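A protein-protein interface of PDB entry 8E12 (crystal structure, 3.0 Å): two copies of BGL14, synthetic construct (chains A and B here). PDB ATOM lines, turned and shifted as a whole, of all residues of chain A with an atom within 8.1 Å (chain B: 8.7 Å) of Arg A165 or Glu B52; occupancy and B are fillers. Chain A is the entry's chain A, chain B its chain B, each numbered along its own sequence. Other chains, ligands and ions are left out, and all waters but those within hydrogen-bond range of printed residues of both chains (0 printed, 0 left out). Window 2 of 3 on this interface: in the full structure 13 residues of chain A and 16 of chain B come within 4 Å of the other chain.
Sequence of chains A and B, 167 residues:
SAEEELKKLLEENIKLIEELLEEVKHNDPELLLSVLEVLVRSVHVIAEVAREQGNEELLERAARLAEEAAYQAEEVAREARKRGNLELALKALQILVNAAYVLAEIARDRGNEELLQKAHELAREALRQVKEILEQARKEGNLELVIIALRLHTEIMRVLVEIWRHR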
ATOM      1  N   TYR A 101      14.018 -13.022   6.589  1.00  0.00           N
ATOM      2  CA  TYR A 101      14.288 -14.353   7.124  1.00  0.00           C
ATOM      3  C   TYR A 101      13.685 -14.521   8.511  1.00  0.00           C
ATOM      4  O   TYR A 101      12.988 -15.507   8.780  1.00  0.00           O
ATOM      5  CB  TYR A 101      15.794 -14.611   7.166  1.00  0.00           C
ATOM      6  CG  TYR A 101      16.152 -16.007   7.630  1.00  0.00           C
ATOM      7  CD1 TYR A 101      16.819 -16.213   8.832  1.00  0.00           C
ATOM      8  CD2 TYR A 101      15.825 -17.119   6.865  1.00  0.00           C
ATOM      9  CE1 TYR A 101      17.146 -17.489   9.259  1.00  0.00           C
ATOM     10  CE2 TYR A 101      16.149 -18.397   7.282  1.00  0.00           C
ATOM     11  CZ  TYR A 101      16.810 -18.577   8.479  1.00  0.00           C
ATOM     12  OH  TYR A 101      17.132 -19.849   8.896  1.00  0.00           O
ATOM     13  N   GLU A 105      10.672 -16.946   9.761  1.00  0.00           N
ATOM     14  CA  GLU A 105      10.806 -17.857  10.893  1.00  0.00           C
ATOM     15  C   GLU A 105       9.720 -17.618  11.935  1.00  0.00           C
ATOM     16  O   GLU A 105       9.154 -18.573  12.482  1.00  0.00           O
ATOM     17  CB  GLU A 105      12.194 -17.712  11.521  1.00  0.00           C
ATOM     18  N   ARG A 108       6.338 -19.027  10.523  1.00  0.00           N
ATOM     19  CA  ARG A 108       6.163 -20.473  10.621  1.00  0.00           C
ATOM     20  C   ARG A 108       5.843 -20.900  12.048  1.00  0.00           C
ATOM     21  O   ARG A 108       5.049 -21.823  12.264  1.00  0.00           O
ATOM     22  CB  ARG A 108       7.416 -21.186  10.113  1.00  0.00           C
ATOM     23  N   LEU A 116       3.856 -15.216   6.437  1.00  0.00           N
ATOM     24  CA  LEU A 116       4.721 -16.042   5.599  1.00  0.00           C
ATOM     25  C   LEU A 116       4.758 -15.537   4.162  1.00  0.00           C
ATOM     26  O   LEU A 116       5.828 -15.489   3.542  1.00  0.00           O
ATOM     27  CB  LEU A 116       4.260 -17.499   5.641  1.00  0.00           C
ATOM     28  CG  LEU A 116       5.281 -18.529   6.130  1.00  0.00           C
ATOM     29  N   MET A 157      17.930 -17.805  -1.211  1.00  0.00           N
ATOM     30  CA  MET A 157      17.527 -19.208  -1.245  1.00  0.00           C
ATOM     31  C   MET A 157      17.285 -19.751   0.158  1.00  0.00           C
ATOM     32  O   MET A 157      16.328 -20.503   0.382  1.00  0.00           O
ATOM     33  CB  MET A 157      18.585 -20.031  -1.974  1.00  0.00           C
ATOM     34  CG  MET A 157      18.361 -20.096  -3.473  1.00  0.00           C
ATOM     35  SD  MET A 157      19.508 -21.183  -4.332  1.00  0.00           S
ATOM     36  CE  MET A 157      20.788 -21.381  -3.104  1.00  0.00           C
ATOM     37  N   ARG A 158      18.147 -19.390   1.113  1.00  0.00           N
ATOM     38  CA  ARG A 158      17.958 -19.833   2.492  1.00  0.00           C
ATOM     39  C   ARG A 158      16.605 -19.388   3.035  1.00  0.00           C
ATOM     40  O   ARG A 158      15.964 -20.121   3.798  1.00  0.00           O
ATOM     41  CB  ARG A 158      19.090 -19.311   3.377  1.00  0.00           C
ATOM     42  CG  ARG A 158      19.825 -20.396   4.151  1.00  0.00           C
ATOM     43  CD  ARG A 158      20.407 -19.852   5.446  1.00  0.00           C
ATOM     44  N   VAL A 159      16.155 -18.189   2.657  1.00  0.00           N
ATOM     45  CA  VAL A 159      14.834 -17.730   3.076  1.00  0.00           C
ATOM     46  C   VAL A 159      13.744 -18.579   2.435  1.00  0.00           C
ATOM     47  O   VAL A 159      12.768 -18.961   3.093  1.00  0.00           O
ATOM     48  CB  VAL A 159      14.658 -16.239   2.736  1.00  0.00           C
ATOM     49  CG1 VAL A 159      13.181 -15.874   2.642  1.00  0.00           C
ATOM     50  CG2 VAL A 159      15.350 -15.384   3.769  1.00  0.00           C
ATOM     51  N   LEU A 160      13.897 -18.899   1.150  1.00  0.00           N
ATOM     52  CA  LEU A 160      12.887 -19.700   0.468  1.00  0.00           C
ATOM     53  C   LEU A 160      12.839 -21.120   1.014  1.00  0.00           C
ATOM     54  O   LEU A 160      11.778 -21.754   0.996  1.00  0.00           O
ATOM     55  CB  LEU A 160      13.145 -19.719  -1.037  1.00  0.00           C
ATOM     56  CG  LEU A 160      12.247 -18.803  -1.872  1.00  0.00           C
ATOM     57  CD1 LEU A 160      12.253 -17.382  -1.322  1.00  0.00           C
ATOM     58  CD2 LEU A 160      12.667 -18.825  -3.330  1.00  0.00           C
ATOM     59  N   VAL A 161      13.973 -21.634   1.494  1.00  0.00           N
ATOM     60  CA  VAL A 161      13.985 -22.964   2.093  1.00  0.00           C
ATOM     61  C   VAL A 161      13.151 -22.983   3.367  1.00  0.00           C
ATOM     62  O   VAL A 161      12.431 -23.951   3.642  1.00  0.00           O
ATOM     63  CB  VAL A 161      15.439 -23.398   2.364  1.00  0.00           C
ATOM     64  CG1 VAL A 161      15.503 -24.449   3.468  1.00  0.00           C
ATOM     65  CG2 VAL A 161      16.106 -23.888   1.092  1.00  0.00           C
ATOM     66  N   GLU A 162      13.207 -21.903   4.152  1.00  0.00           N
ATOM     67  CA  GLU A 162      12.453 -21.857   5.400  1.00  0.00           C
ATOM     68  C   GLU A 162      10.959 -21.697   5.150  1.00  0.00           C
ATOM     69  O   GLU A 162      10.136 -22.266   5.877  1.00  0.00           O
ATOM     70  CB  GLU A 162      12.969 -20.724   6.283  1.00  0.00           C
ATOM     71  CG  GLU A 162      13.361 -21.176   7.674  1.00  0.00           C
ATOM     72  CD  GLU A 162      12.160 -21.580   8.509  1.00  0.00           C
ATOM     73  N   ILE A 163      10.591 -20.905   4.141  1.00  0.00           N
ATOM     74  CA  ILE A 163       9.182 -20.698   3.819  1.00  0.00           C
ATOM     75  C   ILE A 163       8.525 -22.008   3.403  1.00  0.00           C
ATOM     76  O   ILE A 163       7.390 -22.305   3.795  1.00  0.00           O
ATOM     77  CB  ILE A 163       9.054 -19.625   2.725  1.00  0.00           C
ATOM     78  CG1 ILE A 163       9.637 -18.305   3.229  1.00  0.00           C
ATOM     79  CG2 ILE A 163       7.604 -19.452   2.308  1.00  0.00           C
ATOM     80  CD1 ILE A 163       9.449 -17.162   2.283  1.00  0.00           C
ATOM     81  N   TRP A 164       9.231 -22.809   2.603  1.00  0.00           N
ATOM     82  CA  TRP A 164       8.712 -24.112   2.202  1.00  0.00           C
ATOM     83  C   TRP A 164       8.583 -25.031   3.411  1.00  0.00           C
ATOM     84  O   TRP A 164       7.621 -25.801   3.516  1.00  0.00           O
ATOM     85  CB  TRP A 164       9.625 -24.698   1.120  1.00  0.00           C
ATOM     86  CG  TRP A 164       9.610 -26.191   0.891  1.00  0.00           C
ATOM     87  CD1 TRP A 164       8.623 -27.082   1.210  1.00  0.00           C
ATOM     88  CD2 TRP A 164      10.646 -26.955   0.269  1.00  0.00           C
ATOM     89  NE1 TRP A 164       8.986 -28.349   0.830  1.00  0.00           N
ATOM     90  CE2 TRP A 164      10.225 -28.298   0.250  1.00  0.00           C
ATOM     91  CE3 TRP A 164      11.893 -26.630  -0.269  1.00  0.00           C
ATOM     92  CZ2 TRP A 164      11.006 -29.313  -0.286  1.00  0.00           C
ATOM     93  CZ3 TRP A 164      12.663 -27.637  -0.801  1.00  0.00           C
ATOM     94  CH2 TRP A 164      12.219 -28.960  -0.805  1.00  0.00           C
ATOM     95  N   ARG A 165       9.519 -24.928   4.359  1.00  0.00           N
ATOM     96  CA  ARG A 165       9.464 -25.741   5.569  1.00  0.00           C
ATOM     97  C   ARG A 165       8.187 -25.512   6.368  1.00  0.00           C
ATOM     98  O   ARG A 165       7.826 -26.360   7.191  1.00  0.00           O
ATOM     99  CB  ARG A 165      10.675 -25.440   6.453  1.00  0.00           C
ATOM    100  CG  ARG A 165      11.849 -26.382   6.269  1.00  0.00           C
ATOM    101  CD  ARG A 165      12.826 -26.250   7.423  1.00  0.00           C
ATOM    102  NE  ARG A 165      14.056 -25.576   7.027  1.00  0.00           N
ATOM    103  CZ  ARG A 165      14.805 -24.848   7.843  1.00  0.00           C
ATOM    104  NH1 ARG A 165      14.476 -24.676   9.113  1.00  0.00           N
ATOM    105  NH2 ARG A 165      15.908 -24.275   7.372  1.00  0.00           N
ATOM    106  N   HIS A 166       7.497 -24.399   6.145  1.00  0.00           N
ATOM    107  CA  HIS A 166       6.258 -24.111   6.855  1.00  0.00           C
ATOM    108  C   HIS A 166       5.081 -24.827   6.202  1.00  0.00           C
ATOM    109  O   HIS A 166       4.601 -24.416   5.145  1.00  0.00           O
ATOM    110  CB  HIS A 166       5.999 -22.605   6.900  1.00  0.00           C
ATOM    111  N   LEU B   6      11.643 -22.528  -5.408  1.00  0.00           N
ATOM    112  CA  LEU B   6      13.057 -22.578  -5.063  1.00  0.00           C
ATOM    113  C   LEU B   6      13.814 -23.579  -5.926  1.00  0.00           C
ATOM    114  O   LEU B   6      15.021 -23.417  -6.142  1.00  0.00           O
ATOM    115  CB  LEU B   6      13.200 -22.917  -3.582  1.00  0.00           C
ATOM    116  CG  LEU B   6      14.512 -23.510  -3.080  1.00  0.00           C
ATOM    117  CD1 LEU B   6      15.512 -22.412  -2.764  1.00  0.00           C
ATOM    118  CD2 LEU B   6      14.227 -24.357  -1.862  1.00  0.00           C
ATOM    119  N   HIS B  44      26.367 -25.439   1.230  1.00  0.00           N
ATOM    120  CA  HIS B  44      25.753 -25.784   2.508  1.00  0.00           C
ATOM    121  C   HIS B  44      24.232 -25.723   2.433  1.00  0.00           C
ATOM    122  O   HIS B  44      23.544 -26.573   3.011  1.00  0.00           O
ATOM    123  CB  HIS B  44      26.272 -24.865   3.612  1.00  0.00           C
ATOM    124  CG  HIS B  44      26.173 -25.461   4.982  1.00  0.00           C
ATOM    125  ND1 HIS B  44      27.239 -26.066   5.614  1.00  0.00           N
ATOM    126  CD2 HIS B  44      25.130 -25.547   5.841  1.00  0.00           C
ATOM    127  CE1 HIS B  44      26.856 -26.500   6.802  1.00  0.00           C
ATOM    128  NE2 HIS B  44      25.582 -26.197   6.965  1.00  0.00           N
ATOM    129  N   VAL B  45      23.685 -24.733   1.726  1.00  0.00           N
ATOM    130  CA  VAL B  45      22.233 -24.655   1.638  1.00  0.00           C
ATOM    131  C   VAL B  45      21.683 -25.701   0.671  1.00  0.00           C
ATOM    132  O   VAL B  45      20.529 -26.121   0.809  1.00  0.00           O
ATOM    133  CB  VAL B  45      21.774 -23.230   1.271  1.00  0.00           C
ATOM    134  CG1 VAL B  45      22.553 -22.200   2.070  1.00  0.00           C
ATOM    135  CG2 VAL B  45      21.901 -22.978  -0.211  1.00  0.00           C
ATOM    136  N   ILE B  46      22.472 -26.144  -0.314  1.00  0.00           N
ATOM    137  CA  ILE B  46      21.974 -27.221  -1.165  1.00  0.00           C
ATOM    138  C   ILE B  46      21.954 -28.525  -0.380  1.00  0.00           C
ATOM    139  O   ILE B  46      21.112 -29.398  -0.629  1.00  0.00           O
ATOM    140  CB  ILE B  46      22.806 -27.356  -2.457  1.00  0.00           C
ATOM    141  CG1 ILE B  46      23.311 -25.997  -2.948  1.00  0.00           C
ATOM    142  CG2 ILE B  46      21.997 -28.024  -3.547  1.00  0.00           C
ATOM    143  CD1 ILE B  46      22.205 -25.017  -3.297  1.00  0.00           C
ATOM    144  N   ALA B  47      22.879 -28.686   0.572  1.00  0.00           N
ATOM    145  CA  ALA B  47      22.802 -29.808   1.500  1.00  0.00           C
ATOM    146  C   ALA B  47      21.629 -29.634   2.456  1.00  0.00           C
ATOM    147  O   ALA B  47      20.946 -30.605   2.802  1.00  0.00           O
ATOM    148  CB  ALA B  47      24.111 -29.945   2.275  1.00  0.00           C
ATOM    149  N   GLU B  48      21.379 -28.395   2.886  1.00  0.00           N
ATOM    150  CA  GLU B  48      20.266 -28.127   3.790  1.00  0.00           C
ATOM    151  C   GLU B  48      18.926 -28.347   3.104  1.00  0.00           C
ATOM    152  O   GLU B  48      17.934 -28.674   3.768  1.00  0.00           O
ATOM    153  CB  GLU B  48      20.360 -26.700   4.331  1.00  0.00           C
ATOM    154  N   VAL B  49      18.873 -28.189   1.779  1.00  0.00           N
ATOM    155  CA  VAL B  49      17.621 -28.349   1.051  1.00  0.00           C
ATOM    156  C   VAL B  49      17.489 -29.743   0.457  1.00  0.00           C
ATOM    157  O   VAL B  49      16.503 -30.032  -0.233  1.00  0.00           O
ATOM    158  CB  VAL B  49      17.486 -27.273  -0.051  1.00  0.00           C
ATOM    159  CG1 VAL B  49      18.455 -27.532  -1.196  1.00  0.00           C
ATOM    160  CG2 VAL B  49      16.049 -27.128  -0.534  1.00  0.00           C
ATOM    161  N   ALA B  50      18.441 -30.632   0.742  1.00  0.00           N
ATOM    162  CA  ALA B  50      18.345 -32.024   0.344  1.00  0.00           C
ATOM    163  C   ALA B  50      18.104 -32.956   1.519  1.00  0.00           C
ATOM    164  O   ALA B  50      17.698 -34.100   1.303  1.00  0.00           O
ATOM    165  CB  ALA B  50      19.614 -32.460  -0.402  1.00  0.00           C
ATOM    166  N   ARG B  51      18.350 -32.495   2.747  1.00  0.00           N
ATOM    167  CA  ARG B  51      17.895 -33.227   3.922  1.00  0.00           C
ATOM    168  C   ARG B  51      16.404 -33.016   4.146  1.00  0.00           C
ATOM    169  O   ARG B  51      15.700 -33.939   4.573  1.00  0.00           O
ATOM    170  CB  ARG B  51      18.689 -32.794   5.155  1.00  0.00           C
ATOM    171  N   GLU B  52      15.906 -31.809   3.865  1.00  0.00           N
ATOM    172  CA  GLU B  52      14.465 -31.578   3.875  1.00  0.00           C
ATOM    173  C   GLU B  52      13.786 -32.373   2.767  1.00  0.00           C
ATOM    174  O   GLU B  52      12.742 -32.998   2.986  1.00  0.00           O
ATOM    175  CB  GLU B  52      14.170 -30.085   3.730  1.00  0.00           C
ATOM    176  CG  GLU B  52      13.760 -29.400   5.023  1.00  0.00           C
ATOM    177  CD  GLU B  52      14.870 -29.389   6.054  1.00  0.00           C
ATOM    178  OE1 GLU B  52      14.605 -28.991   7.208  1.00  0.00           O
ATOM    179  OE2 GLU B  52      16.009 -29.771   5.712  1.00  0.00           O
ATOM    180  N   GLN B  53      14.362 -32.354   1.568  1.00  0.00           N
ATOM    181  CA  GLN B  53      13.916 -33.238   0.507  1.00  0.00           C
ATOM    182  C   GLN B  53      14.280 -34.683   0.830  1.00  0.00           C
ATOM    183  O   GLN B  53      15.069 -34.975   1.734  1.00  0.00           O
ATOM    184  CB  GLN B  53      14.550 -32.856  -0.832  1.00  0.00           C
ATOM    185  CG  GLN B  53      13.998 -31.614  -1.478  1.00  0.00           C
ATOM    186  CD  GLN B  53      14.820 -31.156  -2.671  1.00  0.00           C
ATOM    187  OE1 GLN B  53      14.439 -31.376  -3.820  1.00  0.00           O
ATOM    188  NE2 GLN B  53      15.948 -30.508  -2.402  1.00  0.00           N
ATOM    189  N   GLY B  54      13.689 -35.594   0.071  1.00  0.00           N
ATOM    190  CA  GLY B  54      14.218 -36.930  -0.066  1.00  0.00           C
ATOM    191  C   GLY B  54      15.243 -37.033  -1.172  1.00  0.00           C
ATOM    192  O   GLY B  54      15.593 -38.142  -1.587  1.00  0.00           O
ATOM    193  N   ASN B  55      15.739 -35.896  -1.652  1.00  0.00           N
ATOM    194  CA  ASN B  55      16.625 -35.826  -2.812  1.00  0.00           C
ATOM    195  C   ASN B  55      18.022 -36.282  -2.416  1.00  0.00           C
ATOM    196  O   ASN B  55      18.792 -35.529  -1.814  1.00  0.00           O
ATOM    197  CB  ASN B  55      16.648 -34.406  -3.366  1.00  0.00           C
ATOM    198  CG  ASN B  55      17.108 -34.348  -4.808  1.00  0.00           C
ATOM    199  OD1 ASN B  55      17.964 -35.123  -5.232  1.00  0.00           O
ATOM    200  ND2 ASN B  55      16.545 -33.418  -5.570  1.00  0.00           N
ATOM    201  N   LEU B  58      20.562 -34.601  -5.198  1.00  0.00           N
ATOM    202  CA  LEU B  58      21.090 -33.270  -4.911  1.00  0.00           C
ATOM    203  C   LEU B  58      22.315 -33.333  -4.009  1.00  0.00           C
ATOM    204  O   LEU B  58      23.193 -32.468  -4.100  1.00  0.00           O
ATOM    205  CB  LEU B  58      20.005 -32.405  -4.275  1.00  0.00           C
ATOM    206  CG  LEU B  58      20.142 -30.900  -4.483  1.00  0.00           C
ATOM    207  CD1 LEU B  58      20.267 -30.567  -5.962  1.00  0.00           C
ATOM    208  CD2 LEU B  58      18.968 -30.162  -3.859  1.00  0.00           C
ATOM    209  N   LEU B  59      22.379 -34.327  -3.119  1.00  0.00           N
ATOM    210  CA  LEU B  59      23.562 -34.503  -2.283  1.00  0.00           C
ATOM    211  C   LEU B  59      24.788 -34.827  -3.127  1.00  0.00           C
ATOM    212  O   LEU B  59      25.888 -34.336  -2.852  1.00  0.00           O
ATOM    213  CB  LEU B  59      23.314 -35.594  -1.245  1.00  0.00           C
ATOM    214  CG  LEU B  59      22.411 -35.205  -0.074  1.00  0.00           C
ATOM    215  CD1 LEU B  59      22.529 -36.218   1.049  1.00  0.00           C
ATOM    216  CD2 LEU B  59      22.768 -33.813   0.425  1.00  0.00           C
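NE of Arg A165 lies within salt-bridge range of OE1 of Glu B52, 3.5 Å away.
OE1 of Gln B53 is in hydrogen-bond range of ND2 of Asn B55, at 3.4 Å.
No position is printed for both chains. Of the 11 pairs that touch across the chains among the printed residues, none has its exchanged pair printed and touching as well.
Met A157 touches Leu B6 (CG to CD1, 3.7 Å). Met A157 touches Val B45 (CE to CG2, 3.5 Å). Met A157 touches Ile B46. CG1 of Val B45 touches CG of Arg A158, at 3.9 Å. CB of Leu A160 touches CD1 of Leu B6 (3.98 Å). Val A161 touches Leu B6 (CG2 to CD2, 3.5 Å). Val A161 touches Val B49 (CG2 to CG2, 3.6 Å). CE3 of Trp A164 touches CD2 of Leu B6, at 3.6 Å. CZ3 of Trp A164 touches CG2 of Val B49, 3.4 Å away. Trp A164 touches Gln B53.
Of chain B, only Glu B52 (3.3 Å) comes within 4 Å of Arg A165. His A166 touches none of the printed residues of chain B. No residue of chain A comes within 4 Å of Arg B51. Of the printed residues of chain A, Val B45 touches Met A157 (3.5 Å) and Arg A158 (3.9 Å). Of the printed residues of chain A, Leu B6 touches Met A157, Leu A160, Val A161 and Trp A164. Printed residues of chain A within 4 Å of Gln B53: Trp A164 (3.3 Å). Gly B54 touches none of the printed residues of chain A. The nearest residue of chain B that does not touch Arg A165 is Glu B48 (5.9 Å). The nearest residue of chain A that does not touch Glu B52 is Trp A164 (5.1 Å).
Printed residues of chain A that touch a printed residue of chain B: Met A157, Arg A158, Leu A160, Val A161, Trp A164 and Arg A165. Along chain A the printed residues that touch a printed residue of chain B span positions 157 to 165. Among the printed residues, Asp or Glu carboxylates within 4 Å of a Lys or Arg side-chain nitrogen of the other chain: Arg A165 with Glu B52 (3.5 Å).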
